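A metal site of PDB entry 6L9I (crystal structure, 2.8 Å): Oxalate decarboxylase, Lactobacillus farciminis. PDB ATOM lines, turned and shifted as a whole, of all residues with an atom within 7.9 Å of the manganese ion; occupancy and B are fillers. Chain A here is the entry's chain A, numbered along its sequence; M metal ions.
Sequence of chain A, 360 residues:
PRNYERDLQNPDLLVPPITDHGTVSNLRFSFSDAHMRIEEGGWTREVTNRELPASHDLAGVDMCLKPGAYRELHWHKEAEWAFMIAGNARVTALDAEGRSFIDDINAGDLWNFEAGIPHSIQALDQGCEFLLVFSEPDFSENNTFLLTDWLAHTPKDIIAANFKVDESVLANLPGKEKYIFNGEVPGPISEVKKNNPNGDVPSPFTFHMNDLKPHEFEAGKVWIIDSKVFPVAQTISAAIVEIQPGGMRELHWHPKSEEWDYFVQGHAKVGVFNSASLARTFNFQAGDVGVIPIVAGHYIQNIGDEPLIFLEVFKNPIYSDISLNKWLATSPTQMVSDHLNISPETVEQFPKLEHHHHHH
The backbone carbonyl oxygen of Glu 250 is in hydrogen-bond range of a ring nitrogen (ND1) of His 252 (2.6 Å).
A ring nitrogen (ND1) of His 254 lies within hydrogen-bond range of the backbone carbonyl oxygen of Ser 320 (3.0 Å).
The backbone carbonyl oxygen (O) of Ala 296 lies within hydrogen-bond range of a ring nitrogen (ND1) of His 298 (2.9 Å).
The backbone carbonyl oxygen of Glu 259 sits at hydrogen-bond distance from the backbone NH of Ile 292 (2.9 Å).
OE2 of Glu 259 lies close to OD1 of Asp 261, 2.6 Å away.
The guanidinium group (NH2) of Arg 249 is in salt-bridge range of the side-chain carboxylate (OE1) of Glu 312 (2.8 Å).
The backbone carbonyl oxygen (O) of Glu 312 sits at hydrogen-bond distance from the backbone NH (N) of Ala 239.
NE2 of His 252 binds the manganese ion (2.2 Å).
NE2 of His 254 binds the manganese ion.
NE2 of His 298 is bound to the manganese ion (2.4 Å).
OE1 of Glu 259 binds the manganese ion, at 2.4 Å.
Slightly farther from the manganese ion lies the side-chain carboxylate (OE2) of Glu 312 (2.9 Å).
Of the 24 residues printed, 5 come within 4 Å of the manganese ion.
The nearest printed residue that does not touch the manganese ion is Arg 249 (4.2 Å).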
ATOM      1  N   ALA A 239      17.295 -36.238   0.520  1.00  0.00           N
ATOM      2  CA  ALA A 239      17.450 -35.185  -0.476  1.00  0.00           C
ATOM      3  C   ALA A 239      18.890 -35.212  -0.955  1.00  0.00           C
ATOM      4  O   ALA A 239      19.810 -35.130  -0.148  1.00  0.00           O
ATOM      5  CB  ALA A 239      17.086 -33.811   0.111  1.00  0.00           C
ATOM      6  N   VAL A 241      21.590 -33.103  -2.753  1.00  0.00           N
ATOM      7  CA  VAL A 241      21.786 -31.676  -2.945  1.00  0.00           C
ATOM      8  C   VAL A 241      23.074 -31.464  -3.717  1.00  0.00           C
ATOM      9  O   VAL A 241      24.117 -32.044  -3.370  1.00  0.00           O
ATOM     10  CB  VAL A 241      21.819 -30.929  -1.588  1.00  0.00           C
ATOM     11  CG1 VAL A 241      21.674 -29.441  -1.803  1.00  0.00           C
ATOM     12  CG2 VAL A 241      20.725 -31.458  -0.670  1.00  0.00           C
ATOM     13  N   ARG A 249      23.549 -23.677   0.721  1.00  0.00           N
ATOM     14  CA  ARG A 249      22.278 -24.202   1.176  1.00  0.00           C
ATOM     15  C   ARG A 249      21.769 -23.243   2.251  1.00  0.00           C
ATOM     16  O   ARG A 249      22.350 -23.170   3.345  1.00  0.00           O
ATOM     17  CB  ARG A 249      22.423 -25.622   1.706  1.00  0.00           C
ATOM     18  CG  ARG A 249      21.120 -26.256   2.161  1.00  0.00           C
ATOM     19  CD  ARG A 249      20.383 -26.942   1.020  1.00  0.00           C
ATOM     20  NE  ARG A 249      19.556 -28.060   1.489  1.00  0.00           N
ATOM     21  CZ  ARG A 249      18.303 -27.937   1.897  1.00  0.00           C
ATOM     22  NH1 ARG A 249      17.714 -26.747   1.890  1.00  0.00           N
ATOM     23  NH2 ARG A 249      17.621 -29.007   2.309  1.00  0.00           N
ATOM     24  N   GLU A 250      20.707 -22.505   1.943  1.00  0.00           N
ATOM     25  CA  GLU A 250      20.321 -21.369   2.755  1.00  0.00           C
ATOM     26  C   GLU A 250      19.933 -21.800   4.173  1.00  0.00           C
ATOM     27  O   GLU A 250      19.640 -22.974   4.435  1.00  0.00           O
ATOM     28  CB  GLU A 250      19.155 -20.621   2.101  1.00  0.00           C
ATOM     29  CG  GLU A 250      17.920 -21.473   1.933  1.00  0.00           C
ATOM     30  CD  GLU A 250      16.811 -20.737   1.244  1.00  0.00           C
ATOM     31  OE1 GLU A 250      16.522 -19.582   1.650  1.00  0.00           O
ATOM     32  OE2 GLU A 250      16.229 -21.293   0.289  1.00  0.00           O
ATOM     33  N   LEU A 251      19.962 -20.837   5.082  1.00  0.00           N
ATOM     34  CA  LEU A 251      19.612 -21.073   6.480  1.00  0.00           C
ATOM     35  C   LEU A 251      18.212 -21.666   6.579  1.00  0.00           C
ATOM     36  O   LEU A 251      17.246 -21.121   6.048  1.00  0.00           O
ATOM     37  CB  LEU A 251      19.688 -19.758   7.262  1.00  0.00           C
ATOM     38  CG  LEU A 251      21.087 -19.232   7.587  1.00  0.00           C
ATOM     39  CD1 LEU A 251      21.031 -17.745   7.881  1.00  0.00           C
ATOM     40  CD2 LEU A 251      21.696 -19.985   8.764  1.00  0.00           C
ATOM     41  N   HIS A 252      18.110 -22.800   7.277  1.00  0.00           N
ATOM     42  CA  HIS A 252      16.873 -23.557   7.344  1.00  0.00           C
ATOM     43  C   HIS A 252      16.952 -24.526   8.501  1.00  0.00           C
ATOM     44  O   HIS A 252      18.001 -24.675   9.144  1.00  0.00           O
ATOM     45  CB  HIS A 252      16.615 -24.311   6.041  1.00  0.00           C
ATOM     46  CG  HIS A 252      17.556 -25.458   5.845  1.00  0.00           C
ATOM     47  ND1 HIS A 252      18.851 -25.297   5.409  1.00  0.00           N
ATOM     48  CD2 HIS A 252      17.390 -26.792   6.042  1.00  0.00           C
ATOM     49  CE1 HIS A 252      19.441 -26.475   5.334  1.00  0.00           C
ATOM     50  NE2 HIS A 252      18.576 -27.405   5.720  1.00  0.00           N
ATOM     51  N   TRP A 253      15.835 -25.208   8.773  1.00  0.00           N
ATOM     52  CA  TRP A 253      15.825 -26.329   9.698  1.00  0.00           C
ATOM     53  C   TRP A 253      14.758 -27.320   9.251  1.00  0.00           C
ATOM     54  O   TRP A 253      13.892 -27.016   8.437  1.00  0.00           O
ATOM     55  CB  TRP A 253      15.580 -25.877  11.149  1.00  0.00           C
ATOM     56  CG  TRP A 253      14.159 -25.560  11.493  1.00  0.00           C
ATOM     57  CD1 TRP A 253      13.189 -26.441  11.880  1.00  0.00           C
ATOM     58  CD2 TRP A 253      13.553 -24.267  11.507  1.00  0.00           C
ATOM     59  NE1 TRP A 253      12.011 -25.771  12.130  1.00  0.00           N
ATOM     60  CE2 TRP A 253      12.208 -24.440  11.903  1.00  0.00           C
ATOM     61  CE3 TRP A 253      14.003 -22.973  11.211  1.00  0.00           C
ATOM     62  CZ2 TRP A 253      11.322 -23.369  12.009  1.00  0.00           C
ATOM     63  CZ3 TRP A 253      13.123 -21.918  11.332  1.00  0.00           C
ATOM     64  CH2 TRP A 253      11.797 -22.122  11.721  1.00  0.00           C
ATOM     65  N   HIS A 254      14.853 -28.528   9.809  1.00  0.00           N
ATOM     66  CA  HIS A 254      13.906 -29.592   9.527  1.00  0.00           C
ATOM     67  C   HIS A 254      13.025 -29.785  10.751  1.00  0.00           C
ATOM     68  O   HIS A 254      13.531 -30.150  11.826  1.00  0.00           O
ATOM     69  CB  HIS A 254      14.631 -30.885   9.165  1.00  0.00           C
ATOM     70  CG  HIS A 254      15.604 -30.718   8.051  1.00  0.00           C
ATOM     71  ND1 HIS A 254      15.242 -30.765   6.718  1.00  0.00           N
ATOM     72  CD2 HIS A 254      16.934 -30.465   8.062  1.00  0.00           C
ATOM     73  CE1 HIS A 254      16.313 -30.559   5.962  1.00  0.00           C
ATOM     74  NE2 HIS A 254      17.343 -30.377   6.754  1.00  0.00           N
ATOM     75  N   GLU A 259      18.984 -34.826  11.148  1.00  0.00           N
ATOM     76  CA  GLU A 259      19.504 -34.953   9.783  1.00  0.00           C
ATOM     77  C   GLU A 259      20.860 -35.646   9.787  1.00  0.00           C
ATOM     78  O   GLU A 259      21.718 -35.370  10.634  1.00  0.00           O
ATOM     79  CB  GLU A 259      19.632 -33.588   9.095  1.00  0.00           C
ATOM     80  CG  GLU A 259      20.388 -33.620   7.780  1.00  0.00           C
ATOM     81  CD  GLU A 259      20.515 -32.249   7.152  1.00  0.00           C
ATOM     82  OE1 GLU A 259      19.675 -31.387   7.443  1.00  0.00           O
ATOM     83  OE2 GLU A 259      21.466 -32.043   6.365  1.00  0.00           O
ATOM     84  N   TRP A 260      21.063 -36.540   8.813  1.00  0.00           N
ATOM     85  CA  TRP A 260      22.267 -37.343   8.655  1.00  0.00           C
ATOM     86  C   TRP A 260      22.830 -37.105   7.265  1.00  0.00           C
ATOM     87  O   TRP A 260      22.119 -37.281   6.266  1.00  0.00           O
ATOM     88  CB  TRP A 260      21.949 -38.824   8.880  1.00  0.00           C
ATOM     89  CG  TRP A 260      23.121 -39.754   9.021  1.00  0.00           C
ATOM     90  CD1 TRP A 260      23.694 -40.183  10.183  1.00  0.00           C
ATOM     91  CD2 TRP A 260      23.835 -40.383   7.952  1.00  0.00           C
ATOM     92  NE1 TRP A 260      24.734 -41.040   9.902  1.00  0.00           N
ATOM     93  CE2 TRP A 260      24.837 -41.178   8.542  1.00  0.00           C
ATOM     94  CE3 TRP A 260      23.726 -40.351   6.564  1.00  0.00           C
ATOM     95  CZ2 TRP A 260      25.733 -41.932   7.780  1.00  0.00           C
ATOM     96  CZ3 TRP A 260      24.612 -41.094   5.810  1.00  0.00           C
ATOM     97  CH2 TRP A 260      25.601 -41.874   6.422  1.00  0.00           C
ATOM     98  N   ASP A 261      24.097 -36.733   7.171  1.00  0.00           N
ATOM     99  CA  ASP A 261      24.702 -36.289   5.927  1.00  0.00           C
ATOM    100  C   ASP A 261      25.756 -37.271   5.440  1.00  0.00           C
ATOM    101  O   ASP A 261      26.440 -37.940   6.228  1.00  0.00           O
ATOM    102  CB  ASP A 261      25.377 -34.928   6.082  1.00  0.00           C
ATOM    103  CG  ASP A 261      24.409 -33.837   6.507  1.00  0.00           C
ATOM    104  OD1 ASP A 261      23.464 -33.581   5.743  1.00  0.00           O
ATOM    105  OD2 ASP A 261      24.611 -33.220   7.574  1.00  0.00           O
ATOM    106  N   ILE A 292      23.051 -33.155  11.958  1.00  0.00           N
ATOM    107  CA  ILE A 292      22.383 -31.936  12.407  1.00  0.00           C
ATOM    108  C   ILE A 292      21.331 -32.347  13.425  1.00  0.00           C
ATOM    109  O   ILE A 292      20.414 -33.095  13.085  1.00  0.00           O
ATOM    110  CB  ILE A 292      21.735 -31.170  11.239  1.00  0.00           C
ATOM    111  CG1 ILE A 292      22.765 -30.844  10.168  1.00  0.00           C
ATOM    112  CG2 ILE A 292      21.051 -29.908  11.760  1.00  0.00           C
ATOM    113  CD1 ILE A 292      23.796 -29.825  10.618  1.00  0.00           C
ATOM    114  N   ALA A 296      17.478 -28.201  14.581  1.00  0.00           N
ATOM    115  CA  ALA A 296      18.593 -27.263  14.635  1.00  0.00           C
ATOM    116  C   ALA A 296      18.664 -26.453  13.349  1.00  0.00           C
ATOM    117  O   ALA A 296      18.424 -26.972  12.253  1.00  0.00           O
ATOM    118  CB  ALA A 296      19.902 -28.010  14.877  1.00  0.00           C
ATOM    119  N   GLY A 297      18.980 -25.168  13.486  1.00  0.00           N
ATOM    120  CA  GLY A 297      19.118 -24.297  12.319  1.00  0.00           C
ATOM    121  C   GLY A 297      20.513 -24.429  11.742  1.00  0.00           C
ATOM    122  O   GLY A 297      21.493 -24.498  12.478  1.00  0.00           O
ATOM    123  N   HIS A 298      20.600 -24.497  10.423  1.00  0.00           N
ATOM    124  CA  HIS A 298      21.926 -24.719   9.860  1.00  0.00           C
ATOM    125  C   HIS A 298      22.021 -24.142   8.454  1.00  0.00           C
ATOM    126  O   HIS A 298      21.019 -23.869   7.786  1.00  0.00           O
ATOM    127  CB  HIS A 298      22.317 -26.207   9.852  1.00  0.00           C
ATOM    128  CG  HIS A 298      21.259 -27.113   9.301  1.00  0.00           C
ATOM    129  ND1 HIS A 298      20.055 -27.343   9.931  1.00  0.00           N
ATOM    130  CD2 HIS A 298      21.257 -27.884   8.184  1.00  0.00           C
ATOM    131  CE1 HIS A 298      19.354 -28.206   9.224  1.00  0.00           C
ATOM    132  NE2 HIS A 298      20.056 -28.553   8.160  1.00  0.00           N
ATOM    133  N   TYR A 299      23.273 -23.956   8.029  1.00  0.00           N
ATOM    134  CA  TYR A 299      23.575 -23.616   6.652  1.00  0.00           C
ATOM    135  C   TYR A 299      24.740 -24.457   6.166  1.00  0.00           C
ATOM    136  O   TYR A 299      25.573 -24.911   6.963  1.00  0.00           O
ATOM    137  CB  TYR A 299      23.923 -22.118   6.506  1.00  0.00           C
ATOM    138  CG  TYR A 299      25.228 -21.766   7.153  1.00  0.00           C
ATOM    139  CD1 TYR A 299      25.286 -21.458   8.502  1.00  0.00           C
ATOM    140  CD2 TYR A 299      26.410 -21.767   6.430  1.00  0.00           C
ATOM    141  CE1 TYR A 299      26.474 -21.139   9.109  1.00  0.00           C
ATOM    142  CE2 TYR A 299      27.614 -21.466   7.031  1.00  0.00           C
ATOM    143  CZ  TYR A 299      27.643 -21.149   8.369  1.00  0.00           C
ATOM    144  OH  TYR A 299      28.841 -20.841   8.967  1.00  0.00           O
ATOM    145  N   ILE A 300      24.818 -24.628   4.843  1.00  0.00           N
ATOM    146  CA  ILE A 300      25.870 -25.394   4.186  1.00  0.00           C
ATOM    147  C   ILE A 300      26.377 -24.573   3.015  1.00  0.00           C
ATOM    148  O   ILE A 300      25.665 -24.397   2.016  1.00  0.00           O
ATOM    149  CB  ILE A 300      25.363 -26.764   3.715  1.00  0.00           C
ATOM    150  CG1 ILE A 300      24.863 -27.600   4.900  1.00  0.00           C
ATOM    151  CG2 ILE A 300      26.460 -27.503   2.952  1.00  0.00           C
ATOM    152  CD1 ILE A 300      23.873 -28.670   4.501  1.00  0.00           C
ATOM    153  N   PHE A 310      25.930 -33.663  -1.720  1.00  0.00           N
ATOM    154  CA  PHE A 310      25.780 -34.424  -0.479  1.00  0.00           C
ATOM    155  C   PHE A 310      24.346 -34.926  -0.351  1.00  0.00           C
ATOM    156  O   PHE A 310      23.443 -34.459  -1.039  1.00  0.00           O
ATOM    157  CB  PHE A 310      26.177 -33.597   0.742  1.00  0.00           C
ATOM    158  CG  PHE A 310      25.440 -32.300   0.875  1.00  0.00           C
ATOM    159  CD1 PHE A 310      24.210 -32.236   1.503  1.00  0.00           C
ATOM    160  CD2 PHE A 310      25.988 -31.128   0.370  1.00  0.00           C
ATOM    161  CE1 PHE A 310      23.531 -31.041   1.626  1.00  0.00           C
ATOM    162  CE2 PHE A 310      25.322 -29.938   0.490  1.00  0.00           C
ATOM    163  CZ  PHE A 310      24.095 -29.886   1.115  1.00  0.00           C
ATOM    164  N   GLU A 312      21.297 -35.372   2.360  1.00  0.00           N
ATOM    165  CA  GLU A 312      20.583 -35.182   3.615  1.00  0.00           C
ATOM    166  C   GLU A 312      19.601 -36.328   3.761  1.00  0.00           C
ATOM    167  O   GLU A 312      18.708 -36.503   2.932  1.00  0.00           O
ATOM    168  CB  GLU A 312      19.844 -33.843   3.618  1.00  0.00           C
ATOM    169  CG  GLU A 312      20.699 -32.616   3.333  1.00  0.00           C
ATOM    170  CD  GLU A 312      19.903 -31.322   3.406  1.00  0.00           C
ATOM    171  OE1 GLU A 312      18.652 -31.379   3.285  1.00  0.00           O
ATOM    172  OE2 GLU A 312      20.500 -30.248   3.596  1.00  0.00           O
ATOM    173  N   VAL A 313      19.753 -37.112   4.825  1.00  0.00           N
ATOM    174  CA  VAL A 313      18.966 -38.314   5.040  1.00  0.00           C
ATOM    175  C   VAL A 313      18.255 -38.203   6.386  1.00  0.00           C
ATOM    176  O   VAL A 313      18.798 -37.617   7.327  1.00  0.00           O
ATOM    177  CB  VAL A 313      19.863 -39.567   4.994  1.00  0.00           C
ATOM    178  CG1 VAL A 313      19.032 -40.842   5.008  1.00  0.00           C
ATOM    179  CG2 VAL A 313      20.766 -39.531   3.777  1.00  0.00           C
ATOM    180  N   PHE A 314      17.040 -38.736   6.457  1.00  0.00           N
ATOM    181  CA  PHE A 314      16.192 -38.577   7.626  1.00  0.00           C
ATOM    182  C   PHE A 314      15.423 -39.867   7.870  1.00  0.00           C
ATOM    183  O   PHE A 314      14.979 -40.518   6.914  1.00  0.00           O
ATOM    184  CB  PHE A 314      15.194 -37.418   7.480  1.00  0.00           C
ATOM    185  CG  PHE A 314      15.778 -36.181   6.845  1.00  0.00           C
ATOM    186  CD1 PHE A 314      15.921 -36.074   5.471  1.00  0.00           C
ATOM    187  CD2 PHE A 314      16.174 -35.112   7.633  1.00  0.00           C
ATOM    188  CE1 PHE A 314      16.452 -34.931   4.895  1.00  0.00           C
ATOM    189  CE2 PHE A 314      16.709 -33.961   7.063  1.00  0.00           C
ATOM    190  CZ  PHE A 314      16.844 -33.878   5.688  1.00  0.00           C
ATOM    191  N   TYR A 319       9.821 -35.847   3.582  1.00  0.00           N
ATOM    192  CA  TYR A 319      10.770 -34.749   3.690  1.00  0.00           C
ATOM    193  C   TYR A 319      10.041 -33.463   4.046  1.00  0.00           C
ATOM    194  O   TYR A 319       8.934 -33.197   3.562  1.00  0.00           O
ATOM    195  CB  TYR A 319      11.561 -34.549   2.395  1.00  0.00           C
ATOM    196  CG  TYR A 319      12.480 -33.331   2.446  1.00  0.00           C
ATOM    197  CD1 TYR A 319      12.019 -32.067   2.099  1.00  0.00           C
ATOM    198  CD2 TYR A 319      13.811 -33.448   2.858  1.00  0.00           C
ATOM    199  CE1 TYR A 319      12.842 -30.952   2.162  1.00  0.00           C
ATOM    200  CE2 TYR A 319      14.641 -32.340   2.925  1.00  0.00           C
ATOM    201  CZ  TYR A 319      14.149 -31.096   2.569  1.00  0.00           C
ATOM    202  OH  TYR A 319      14.978 -29.988   2.637  1.00  0.00           O
ATOM    203  N   SER A 320      10.666 -32.661   4.902  1.00  0.00           N
ATOM    204  CA  SER A 320      10.156 -31.342   5.209  1.00  0.00           C
ATOM    205  C   SER A 320      11.315 -30.488   5.681  1.00  0.00           C
ATOM    206  O   SER A 320      12.248 -30.979   6.331  1.00  0.00           O
ATOM    207  CB  SER A 320       9.050 -31.392   6.278  1.00  0.00           C
ATOM    208  OG  SER A 320       9.513 -31.969   7.479  1.00  0.00           O
ATOM    209  N   ASP A 321      11.265 -29.215   5.335  1.00  0.00           N
ATOM    210  CA  ASP A 321      12.187 -28.237   5.896  1.00  0.00           C
ATOM    211  C   ASP A 321      11.489 -26.889   5.898  1.00  0.00           C
ATOM    212  O   ASP A 321      10.424 -26.719   5.289  1.00  0.00           O
ATOM    213  CB  ASP A 321      13.531 -28.206   5.140  1.00  0.00           C
ATOM    214  CG  ASP A 321      13.478 -27.392   3.837  1.00  0.00           C
ATOM    215  OD1 ASP A 321      12.384 -27.177   3.274  1.00  0.00           O
ATOM    216  OD2 ASP A 321      14.566 -26.993   3.372  1.00  0.00           O
HETATM  217 MN    MN M   1      19.280 -29.437   6.122  1.00  0.00          MN
